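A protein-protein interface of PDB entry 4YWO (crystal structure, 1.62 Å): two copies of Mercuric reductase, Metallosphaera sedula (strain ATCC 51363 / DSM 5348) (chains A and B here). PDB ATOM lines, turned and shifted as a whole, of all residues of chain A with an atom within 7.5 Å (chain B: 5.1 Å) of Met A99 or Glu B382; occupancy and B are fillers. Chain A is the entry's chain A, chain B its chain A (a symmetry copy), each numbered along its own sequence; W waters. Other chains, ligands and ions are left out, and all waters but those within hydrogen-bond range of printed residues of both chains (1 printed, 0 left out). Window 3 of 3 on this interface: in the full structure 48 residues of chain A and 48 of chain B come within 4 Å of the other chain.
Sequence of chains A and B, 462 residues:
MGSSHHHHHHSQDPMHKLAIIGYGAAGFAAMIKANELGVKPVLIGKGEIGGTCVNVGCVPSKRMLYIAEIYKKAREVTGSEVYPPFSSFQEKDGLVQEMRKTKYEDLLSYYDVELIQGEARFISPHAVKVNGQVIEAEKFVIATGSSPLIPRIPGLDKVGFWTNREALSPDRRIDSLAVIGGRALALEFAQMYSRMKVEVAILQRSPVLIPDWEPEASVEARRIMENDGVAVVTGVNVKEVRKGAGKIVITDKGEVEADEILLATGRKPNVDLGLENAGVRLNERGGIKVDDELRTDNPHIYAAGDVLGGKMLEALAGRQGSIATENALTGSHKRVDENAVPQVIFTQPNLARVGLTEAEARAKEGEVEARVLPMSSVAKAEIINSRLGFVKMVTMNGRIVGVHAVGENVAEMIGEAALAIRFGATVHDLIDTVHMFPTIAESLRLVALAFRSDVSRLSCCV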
ATOM      1  N   CYS A  53      11.601  29.195 -14.899  1.00  0.00           N
ATOM      2  CA  CYS A  53      12.245  28.309 -13.938  1.00  0.00           C
ATOM      3  C   CYS A  53      11.331  27.909 -12.790  1.00  0.00           C
ATOM      4  O   CYS A  53      11.108  26.723 -12.547  1.00  0.00           O
ATOM      5  CB  CYS A  53      13.518  28.958 -13.387  1.00  0.00           C
ATOM      6  SG  CYS A  53      14.363  27.987 -12.117  1.00  0.00           S
ATOM      7  N   VAL A  54      10.810  28.903 -12.082  1.00  0.00           N
ATOM      8  CA  VAL A  54      10.011  28.638 -10.898  1.00  0.00           C
ATOM      9  C   VAL A  54       8.657  28.099 -11.225  1.00  0.00           C
ATOM     10  O   VAL A  54       8.061  27.339 -10.474  1.00  0.00           O
ATOM     11  CB  VAL A  54      10.006  29.855  -9.928  1.00  0.00           C
ATOM     12  CG1 VAL A  54       9.141  30.996 -10.432  1.00  0.00           C
ATOM     13  CG2 VAL A  54       9.534  29.433  -8.567  1.00  0.00           C
ATOM     14  N   VAL A  59      11.924  24.098 -11.172  1.00  0.00           N
ATOM     15  CA  VAL A  59      11.378  23.795  -9.835  1.00  0.00           C
ATOM     16  C   VAL A  59      10.269  22.716  -9.852  1.00  0.00           C
ATOM     17  O   VAL A  59      10.396  21.674  -9.180  1.00  0.00           O
ATOM     18  CB  VAL A  59      10.926  25.070  -9.118  1.00  0.00           C
ATOM     19  CG1 VAL A  59      10.158  24.753  -7.899  1.00  0.00           C
ATOM     20  CG2 VAL A  59      12.161  25.907  -8.853  1.00  0.00           C
ATOM     21  N   PRO A  60       9.195  22.874 -10.683  1.00  0.00           N
ATOM     22  CA  PRO A  60       8.185  21.837 -10.659  1.00  0.00           C
ATOM     23  C   PRO A  60       8.699  20.484 -11.273  1.00  0.00           C
ATOM     24  O   PRO A  60       8.284  19.390 -10.792  1.00  0.00           O
ATOM     25  CB  PRO A  60       7.087  22.400 -11.600  1.00  0.00           C
ATOM     26  CG  PRO A  60       7.762  23.553 -12.274  1.00  0.00           C
ATOM     27  CD  PRO A  60       8.726  24.093 -11.388  1.00  0.00           C
ATOM     28  N   ARG A  63      10.775  18.698  -8.648  1.00  0.00           N
ATOM     29  CA  ARG A  63       9.905  18.173  -7.616  1.00  0.00           C
ATOM     30  C   ARG A  63       9.256  16.888  -8.063  1.00  0.00           C
ATOM     31  O   ARG A  63       9.188  15.906  -7.297  1.00  0.00           O
ATOM     32  CB  ARG A  63       8.859  19.211  -7.198  1.00  0.00           C
ATOM     33  CG  ARG A  63       7.802  18.683  -6.233  1.00  0.00           C
ATOM     34  CD  ARG A  63       8.458  18.341  -4.867  1.00  0.00           C
ATOM     35  NE  ARG A  63       7.417  18.155  -3.903  1.00  0.00           N
ATOM     36  CZ  ARG A  63       7.654  17.866  -2.644  1.00  0.00           C
ATOM     37  NH1 ARG A  63       8.887  17.745  -2.183  1.00  0.00           N
ATOM     38  NH2 ARG A  63       6.600  17.620  -1.852  1.00  0.00           N
ATOM     39  N   TYR A  66      11.649  14.003  -8.016  1.00  0.00           N
ATOM     40  CA  TYR A  66      11.926  13.596  -6.601  1.00  0.00           C
ATOM     41  C   TYR A  66      10.829  12.639  -6.127  1.00  0.00           C
ATOM     42  O   TYR A  66      11.111  11.537  -5.608  1.00  0.00           O
ATOM     43  CB  TYR A  66      12.091  14.796  -5.717  1.00  0.00           C
ATOM     44  CG  TYR A  66      12.038  14.440  -4.246  1.00  0.00           C
ATOM     45  CD1 TYR A  66      13.100  13.848  -3.671  1.00  0.00           C
ATOM     46  CD2 TYR A  66      10.900  14.716  -3.481  1.00  0.00           C
ATOM     47  CE1 TYR A  66      13.025  13.527  -2.321  1.00  0.00           C
ATOM     48  CE2 TYR A  66      10.832  14.392  -2.149  1.00  0.00           C
ATOM     49  CZ  TYR A  66      11.866  13.742  -1.624  1.00  0.00           C
ATOM     50  OH  TYR A  66      11.734  13.449  -0.238  1.00  0.00           O
ATOM     51  N   ASP A  93       2.016  22.367  -6.730  1.00  0.00           N
ATOM     52  CA  ASP A  93       1.634  23.787  -6.987  1.00  0.00           C
ATOM     53  C   ASP A  93       1.779  24.661  -5.723  1.00  0.00           C
ATOM     54  O   ASP A  93       2.203  25.802  -5.787  1.00  0.00           O
ATOM     55  CB  ASP A  93       0.192  23.877  -7.476  1.00  0.00           C
ATOM     56  CG  ASP A  93      -0.025  23.290  -8.858  1.00  0.00           C
ATOM     57  OD1 ASP A  93       0.892  23.080  -9.666  1.00  0.00           O
ATOM     58  OD2 ASP A  93      -1.215  23.096  -9.180  1.00  0.00           O
ATOM     59  N   GLY A  94       1.606  24.081  -4.559  1.00  0.00           N
ATOM     60  CA  GLY A  94       1.922  24.790  -3.324  1.00  0.00           C
ATOM     61  C   GLY A  94       3.371  25.237  -3.119  1.00  0.00           C
ATOM     62  O   GLY A  94       3.652  26.343  -2.641  1.00  0.00           O
ATOM     63  N   LEU A  95       4.301  24.342  -3.476  1.00  0.00           N
ATOM     64  CA  LEU A  95       5.728  24.636  -3.392  1.00  0.00           C
ATOM     65  C   LEU A  95       6.078  25.728  -4.416  1.00  0.00           C
ATOM     66  O   LEU A  95       6.819  26.649  -4.095  1.00  0.00           O
ATOM     67  CB  LEU A  95       6.511  23.332  -3.682  1.00  0.00           C
ATOM     68  CG  LEU A  95       7.988  23.568  -3.849  1.00  0.00           C
ATOM     69  CD1 LEU A  95       8.656  24.017  -2.568  1.00  0.00           C
ATOM     70  CD2 LEU A  95       8.628  22.249  -4.290  1.00  0.00           C
ATOM     71  N   VAL A  96       5.519  25.644  -5.617  1.00  0.00           N
ATOM     72  CA  VAL A  96       5.775  26.617  -6.670  1.00  0.00           C
ATOM     73  C   VAL A  96       5.338  27.987  -6.149  1.00  0.00           C
ATOM     74  O   VAL A  96       6.037  29.003  -6.211  1.00  0.00           O
ATOM     75  CB  VAL A  96       5.065  26.252  -7.994  1.00  0.00           C
ATOM     76  CG1 VAL A  96       5.098  27.403  -8.965  1.00  0.00           C
ATOM     77  CG2 VAL A  96       5.747  25.045  -8.629  1.00  0.00           C
ATOM     78  N   GLN A  97       4.116  28.032  -5.642  1.00  0.00           N
ATOM     79  CA  GLN A  97       3.585  29.329  -5.063  1.00  0.00           C
ATOM     80  C   GLN A  97       4.367  29.942  -3.956  1.00  0.00           C
ATOM     81  O   GLN A  97       4.655  31.149  -3.930  1.00  0.00           O
ATOM     82  CB  GLN A  97       2.125  29.108  -4.619  1.00  0.00           C
ATOM     83  CG  GLN A  97       1.246  28.865  -5.851  1.00  0.00           C
ATOM     84  CD  GLN A  97      -0.152  28.336  -5.521  1.00  0.00           C
ATOM     85  OE1 GLN A  97      -0.617  28.436  -4.370  1.00  0.00           O
ATOM     86  NE2 GLN A  97      -0.818  27.756  -6.528  1.00  0.00           N
ATOM     87  N   GLU A  98       4.829  29.093  -3.025  1.00  0.00           N
ATOM     88  CA  GLU A  98       5.686  29.514  -1.975  1.00  0.00           C
ATOM     89  C   GLU A  98       7.030  29.999  -2.495  1.00  0.00           C
ATOM     90  O   GLU A  98       7.527  31.056  -2.086  1.00  0.00           O
ATOM     91  CB  GLU A  98       5.962  28.366  -0.972  1.00  0.00           C
ATOM     92  CG  GLU A  98       7.004  28.757   0.080  1.00  0.00           C
ATOM     93  CD  GLU A  98       7.891  27.607   0.642  1.00  0.00           C
ATOM     94  OE1 GLU A  98       8.741  27.950   1.480  1.00  0.00           O
ATOM     95  OE2 GLU A  98       7.776  26.389   0.317  1.00  0.00           O
ATOM     96  N   MET A  99       7.629  29.260  -3.414  1.00  0.00           N
ATOM     97  CA  MET A  99       8.919  29.703  -3.904  1.00  0.00           C
ATOM     98  C   MET A  99       8.839  30.976  -4.764  1.00  0.00           C
ATOM     99  O   MET A  99       9.726  31.806  -4.739  1.00  0.00           O
ATOM    100  CB  MET A  99       9.601  28.559  -4.642  1.00  0.00           C
ATOM    101  CG  MET A  99       9.904  27.413  -3.700  1.00  0.00           C
ATOM    102  SD  MET A  99      10.850  25.986  -4.419  1.00  0.00           S
ATOM    103  CE  MET A  99      11.901  27.156  -5.280  1.00  0.00           C
ATOM    104  N   ARG A 100       7.755  31.107  -5.506  1.00  0.00           N
ATOM    105  CA  ARG A 100       7.505  32.287  -6.370  1.00  0.00           C
ATOM    106  C   ARG A 100       7.397  33.505  -5.444  1.00  0.00           C
ATOM    107  O   ARG A 100       7.990  34.571  -5.690  1.00  0.00           O
ATOM    108  CB  ARG A 100       6.311  32.133  -7.265  1.00  0.00           C
ATOM    109  CG  ARG A 100       6.101  33.316  -8.213  1.00  0.00           C
ATOM    110  CD  ARG A 100       4.644  33.391  -8.626  1.00  0.00           C
ATOM    111  NE  ARG A 100       4.243  32.230  -9.306  1.00  0.00           N
ATOM    112  CZ  ARG A 100       3.107  31.573  -9.124  1.00  0.00           C
ATOM    113  NH1 ARG A 100       2.199  31.870  -8.199  1.00  0.00           N
ATOM    114  NH2 ARG A 100       2.947  30.549  -9.869  1.00  0.00           N
ATOM    115  N   LYS A 101       6.708  33.326  -4.329  1.00  0.00           N
ATOM    116  CA  LYS A 101       6.591  34.425  -3.351  1.00  0.00           C
ATOM    117  C   LYS A 101       7.921  34.800  -2.722  1.00  0.00           C
ATOM    118  O   LYS A 101       8.358  35.945  -2.802  1.00  0.00           O
ATOM    119  CB  LYS A 101       5.529  34.142  -2.295  1.00  0.00           C
ATOM    120  CG  LYS A 101       5.296  35.320  -1.340  1.00  0.00           C
ATOM    121  CD  LYS A 101       4.048  35.074  -0.531  1.00  0.00           C
ATOM    122  CE  LYS A 101       3.702  36.311   0.317  1.00  0.00           C
ATOM    123  NZ  LYS A 101       4.857  36.694   1.210  1.00  0.00           N
ATOM    124  N   THR A 102       8.633  33.846  -2.148  1.00  0.00           N
ATOM    125  CA  THR A 102       9.806  34.154  -1.343  1.00  0.00           C
ATOM    126  C   THR A 102      11.007  34.607  -2.165  1.00  0.00           C
ATOM    127  O   THR A 102      11.732  35.507  -1.770  1.00  0.00           O
ATOM    128  CB  THR A 102      10.200  32.923  -0.453  1.00  0.00           C
ATOM    129  OG1 THR A 102      10.450  31.779  -1.278  1.00  0.00           O
ATOM    130  CG2 THR A 102       9.092  32.565   0.402  1.00  0.00           C
ATOM    131  N   LYS A 103      11.142  34.043  -3.362  1.00  0.00           N
ATOM    132  CA  LYS A 103      12.288  34.239  -4.240  1.00  0.00           C
ATOM    133  C   LYS A 103      12.108  35.316  -5.309  1.00  0.00           C
ATOM    134  O   LYS A 103      13.105  35.730  -5.938  1.00  0.00           O
ATOM    135  CB  LYS A 103      12.695  32.917  -4.907  1.00  0.00           C
ATOM    136  CG  LYS A 103      12.955  31.769  -3.916  1.00  0.00           C
ATOM    137  CD  LYS A 103      14.366  31.802  -3.329  1.00  0.00           C
ATOM    138  CE  LYS A 103      14.715  33.106  -2.600  1.00  0.00           C
ATOM    139  NZ  LYS A 103      15.916  33.014  -1.719  1.00  0.00           N
ATOM    140  N   TYR A 104      10.870  35.714  -5.579  1.00  0.00           N
ATOM    141  CA  TYR A 104      10.578  36.694  -6.630  1.00  0.00           C
ATOM    142  C   TYR A 104       9.612  37.784  -6.189  1.00  0.00           C
ATOM    143  O   TYR A 104      10.031  38.907  -6.116  1.00  0.00           O
ATOM    144  CB  TYR A 104      10.025  35.998  -7.889  1.00  0.00           C
ATOM    145  CG  TYR A 104      11.037  34.997  -8.446  1.00  0.00           C
ATOM    146  CD1 TYR A 104      12.085  35.429  -9.271  1.00  0.00           C
ATOM    147  CD2 TYR A 104      10.957  33.677  -8.126  1.00  0.00           C
ATOM    148  CE1 TYR A 104      12.985  34.574  -9.766  1.00  0.00           C
ATOM    149  CE2 TYR A 104      11.864  32.784  -8.652  1.00  0.00           C
ATOM    150  CZ  TYR A 104      12.853  33.220  -9.463  1.00  0.00           C
ATOM    151  OH  TYR A 104      13.825  32.329  -9.979  1.00  0.00           O
ATOM    152  N   GLU A 105       8.361  37.455  -5.832  1.00  0.00           N
ATOM    153  CA  GLU A 105       7.408  38.501  -5.504  1.00  0.00           C
ATOM    154  C   GLU A 105       7.885  39.319  -4.315  1.00  0.00           C
ATOM    155  O   GLU A 105       7.750  40.577  -4.285  1.00  0.00           O
ATOM    156  CB  GLU A 105       6.019  37.912  -5.225  1.00  0.00           C
ATOM    157  CG  GLU A 105       5.367  37.313  -6.486  1.00  0.00           C
ATOM    158  CD  GLU A 105       4.204  36.279  -6.317  1.00  0.00           C
ATOM    159  OE1 GLU A 105       3.933  35.786  -5.217  1.00  0.00           O
ATOM    160  OE2 GLU A 105       3.570  35.946  -7.352  1.00  0.00           O
ATOM    161  N   ASP A 106       8.463  38.684  -3.313  1.00  0.00           N
ATOM    162  CA  ASP A 106       8.871  39.464  -2.148  1.00  0.00           C
ATOM    163  C   ASP A 106      10.025  40.408  -2.498  1.00  0.00           C
ATOM    164  O   ASP A 106      10.233  41.410  -1.830  1.00  0.00           O
ATOM    165  CB  ASP A 106       9.310  38.570  -0.976  1.00  0.00           C
ATOM    166  CG  ASP A 106       8.112  37.916  -0.217  1.00  0.00           C
ATOM    167  OD1 ASP A 106       6.924  38.243  -0.410  1.00  0.00           O
ATOM    168  OD2 ASP A 106       8.421  37.003   0.569  1.00  0.00           O
ATOM    169  N   SER B 376      17.154  25.809   4.663  1.00  0.00           N
ATOM    170  CA  SER B 376      15.784  26.060   4.320  1.00  0.00           C
ATOM    171  C   SER B 376      15.710  27.093   3.205  1.00  0.00           C
ATOM    172  O   SER B 376      14.669  27.051   2.530  1.00  0.00           O
ATOM    173  CB  SER B 376      15.044  26.527   5.618  1.00  0.00           C
ATOM    174  OG  SER B 376      15.531  27.737   6.026  1.00  0.00           O
ATOM    175  N   SER B 377      16.758  27.915   2.967  1.00  0.00           N
ATOM    176  CA  SER B 377      16.909  28.944   1.893  1.00  0.00           C
ATOM    177  C   SER B 377      17.411  28.331   0.558  1.00  0.00           C
ATOM    178  O   SER B 377      17.502  29.090  -0.433  1.00  0.00           O
ATOM    179  CB  SER B 377      17.948  29.978   2.222  1.00  0.00           C
ATOM    180  OG  SER B 377      17.388  30.817   3.298  1.00  0.00           O
ATOM    181  N   VAL B 378      17.750  27.056   0.525  1.00  0.00           N
ATOM    182  CA  VAL B 378      18.333  26.461  -0.679  1.00  0.00           C
ATOM    183  C   VAL B 378      17.245  25.801  -1.485  1.00  0.00           C
ATOM    184  O   VAL B 378      16.545  24.894  -0.959  1.00  0.00           O
ATOM    185  CB  VAL B 378      19.450  25.465  -0.224  1.00  0.00           C
ATOM    186  CG1 VAL B 378      20.087  24.756  -1.400  1.00  0.00           C
ATOM    187  CG2 VAL B 378      20.542  26.234   0.515  1.00  0.00           C
ATOM    188  N   ALA B 379      17.007  26.193  -2.754  1.00  0.00           N
ATOM    189  CA  ALA B 379      15.874  25.658  -3.471  1.00  0.00           C
ATOM    190  C   ALA B 379      15.844  24.161  -3.485  1.00  0.00           C
ATOM    191  O   ALA B 379      14.822  23.582  -3.260  1.00  0.00           O
ATOM    192  CB  ALA B 379      15.871  26.125  -4.938  1.00  0.00           C
ATOM    193  N   LYS B 380      16.990  23.514  -3.773  1.00  0.00           N
ATOM    194  CA  LYS B 380      16.924  22.084  -3.904  1.00  0.00           C
ATOM    195  C   LYS B 380      16.501  21.410  -2.584  1.00  0.00           C
ATOM    196  O   LYS B 380      15.837  20.407  -2.555  1.00  0.00           O
ATOM    197  CB  LYS B 380      18.291  21.504  -4.391  1.00  0.00           C
ATOM    198  CG  LYS B 380      18.240  20.010  -4.691  1.00  0.00           C
ATOM    199  CD  LYS B 380      17.141  19.692  -5.732  1.00  0.00           C
ATOM    200  CE  LYS B 380      17.195  18.362  -6.452  1.00  0.00           C
ATOM    201  NZ  LYS B 380      18.378  18.287  -7.356  1.00  0.00           N
ATOM    202  N   ALA B 381      16.945  21.972  -1.466  1.00  0.00           N
ATOM    203  CA  ALA B 381      16.600  21.418  -0.131  1.00  0.00           C
ATOM    204  C   ALA B 381      15.075  21.508   0.103  1.00  0.00           C
ATOM    205  O   ALA B 381      14.443  20.548   0.612  1.00  0.00           O
ATOM    206  CB  ALA B 381      17.355  22.130   0.977  1.00  0.00           C
ATOM    207  N   GLU B 382      14.427  22.565  -0.399  1.00  0.00           N
ATOM    208  CA  GLU B 382      12.979  22.653  -0.381  1.00  0.00           C
ATOM    209  C   GLU B 382      12.314  21.622  -1.284  1.00  0.00           C
ATOM    210  O   GLU B 382      11.336  20.909  -0.898  1.00  0.00           O
ATOM    211  CB  GLU B 382      12.599  24.118  -0.742  1.00  0.00           C
ATOM    212  CG  GLU B 382      13.225  25.187   0.155  1.00  0.00           C
ATOM    213  CD  GLU B 382      13.124  26.674  -0.304  1.00  0.00           C
ATOM    214  OE1 GLU B 382      12.017  27.002  -0.786  1.00  0.00           O
ATOM    215  OE2 GLU B 382      14.158  27.456  -0.209  1.00  0.00           O
ATOM    216  N   ILE B 383      12.862  21.440  -2.470  1.00  0.00           N
ATOM    217  CA  ILE B 383      12.322  20.512  -3.464  1.00  0.00           C
ATOM    218  C   ILE B 383      12.330  19.045  -2.999  1.00  0.00           C
ATOM    219  O   ILE B 383      11.360  18.306  -3.190  1.00  0.00           O
ATOM    220  CB  ILE B 383      13.068  20.658  -4.820  1.00  0.00           C
ATOM    221  CG1 ILE B 383      12.753  22.003  -5.463  1.00  0.00           C
ATOM    222  CG2 ILE B 383      12.770  19.495  -5.812  1.00  0.00           C
ATOM    223  CD1 ILE B 383      13.692  22.377  -6.593  1.00  0.00           C
ATOM    224  N   ILE B 384      13.373  18.673  -2.239  1.00  0.00           N
ATOM    225  CA  ILE B 384      13.526  17.292  -1.784  1.00  0.00           C
ATOM    226  C   ILE B 384      13.175  17.092  -0.321  1.00  0.00           C
ATOM    227  O   ILE B 384      13.565  16.079   0.255  1.00  0.00           O
ATOM    228  CB  ILE B 384      14.961  16.768  -2.119  1.00  0.00           C
ATOM    229  CG1 ILE B 384      16.055  17.440  -1.264  1.00  0.00           C
ATOM    230  CG2 ILE B 384      15.292  16.843  -3.595  1.00  0.00           C
ATOM    231  CD1 ILE B 384      17.489  16.971  -1.405  1.00  0.00           C
ATOM    232  N   ASN B 385      12.497  18.056   0.254  1.00  0.00           N
ATOM    233  CA  ASN B 385      12.004  17.935   1.634  1.00  0.00           C
ATOM    234  C   ASN B 385      13.135  17.680   2.629  1.00  0.00           C
ATOM    235  O   ASN B 385      13.059  16.766   3.480  1.00  0.00           O
ATOM    236  CB  ASN B 385      10.943  16.801   1.705  1.00  0.00           C
ATOM    237  CG  ASN B 385       9.630  17.198   1.078  1.00  0.00           C
ATOM    238  OD1 ASN B 385       9.428  18.363   0.738  1.00  0.00           O
ATOM    239  ND2 ASN B 385       8.706  16.228   0.914  1.00  0.00           N
ATOM    240  N   SER B 386      14.229  18.442   2.501  1.00  0.00           N
ATOM    241  CA  SER B 386      15.376  18.257   3.419  1.00  0.00           C
ATOM    242  C   SER B 386      15.881  19.587   3.877  1.00  0.00           C
ATOM    243  O   SER B 386      16.990  20.039   3.619  1.00  0.00           O
ATOM    244  CB  SER B 386      16.450  17.405   2.714  1.00  0.00           C
ATOM    245  OG  SER B 386      17.399  17.012   3.726  1.00  0.00           O
ATOM    246  N   ARG B 387      14.998  20.304   4.572  1.00  0.00           N
ATOM    247  CA  ARG B 387      15.286  21.687   4.897  1.00  0.00           C
ATOM    248  C   ARG B 387      16.136  21.870   6.169  1.00  0.00           C
ATOM    249  O   ARG B 387      16.659  22.976   6.329  1.00  0.00           O
ATOM    250  CB  ARG B 387      13.959  22.476   5.114  1.00  0.00           C
ATOM    251  CG  ARG B 387      13.143  22.571   3.830  1.00  0.00           C
ATOM    252  CD  ARG B 387      11.858  23.269   4.194  1.00  0.00           C
ATOM    253  NE  ARG B 387      11.124  23.786   3.089  1.00  0.00           N
ATOM    254  CZ  ARG B 387      10.309  23.142   2.277  1.00  0.00           C
ATOM    255  NH1 ARG B 387      10.202  21.775   2.283  1.00  0.00           N
ATOM    256  NH2 ARG B 387       9.624  23.920   1.383  1.00  0.00           N
HETATM  257  O   HOH W   1       9.486  13.575   1.150  1.00  0.00           O
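Water W1 bridges OH of Tyr A66 (2.6 Å) and ND2 of Asn B385 (2.8 Å).
The side-chain carboxylate (OE2) of Glu A98 is in salt-bridge range of the guanidinium group (NH2) of Arg B387. The side-chain hydroxyl (OH) of Tyr A66 is in hydrogen-bond range of the backbone carbonyl oxygen (O) of Ile B384, at 3.2 Å. NH1 of Arg A63 is in hydrogen-bond range of OD1 of Asn B385 (3.0 Å). The guanidinium group (NH1) of Arg A63 lies within hydrogen-bond range of the backbone carbonyl oxygen (O) of Ile B383 (2.7 Å).
Tyr A66 touches Ile B383. Tyr A66 touches Asn B385. Glu B382 touches Met A99 (OE1 to CG, 3.6 Å).
Of the printed residues of chain B, Arg A63 touches Ile B383 and Asn B385. Of the printed residues of chain B, Tyr A66 touches Ile B383 (3.6 Å), Ile B384 (3.2 Å) and Asn B385 (3.95 Å). Met A99 touches one residue of chain B. Glu A105 touches none of the printed residues of chain B. Ser B377 touches none of the printed residues of chain A. No residue of chain A comes within 4 Å of Ala B381. Glu B382 touches one residue of chain A. Printed residues of chain A within 4 Å of Ile B383: Arg A63 and Tyr A66. The nearest printed residue of chain A that does not touch Arg B387 is Leu A95 (4.1 Å).
No position is printed for both chains.
Printed residues of chain B that touch a printed residue of chain A: Glu B382, Ile B383, Ile B384, Asn B385 and Arg B387. Of the 20 printed residues of chain A, 4 touch a printed residue of chain B. Hydrophobic or aromatic side chains of chain A that line the printed part of chain B: Tyr A66 and Met A99.
O of Glu A98 is in hydrogen-bond range of OG1 of Thr A102. O of Glu B382 sits at hydrogen-bond distance from NH1 of Arg B387, at 3.5 Å. The backbone NH (N) of Ser B376 sits at hydrogen-bond distance from the backbone carbonyl oxygen (O) of Arg B387, 3.3 Å away.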
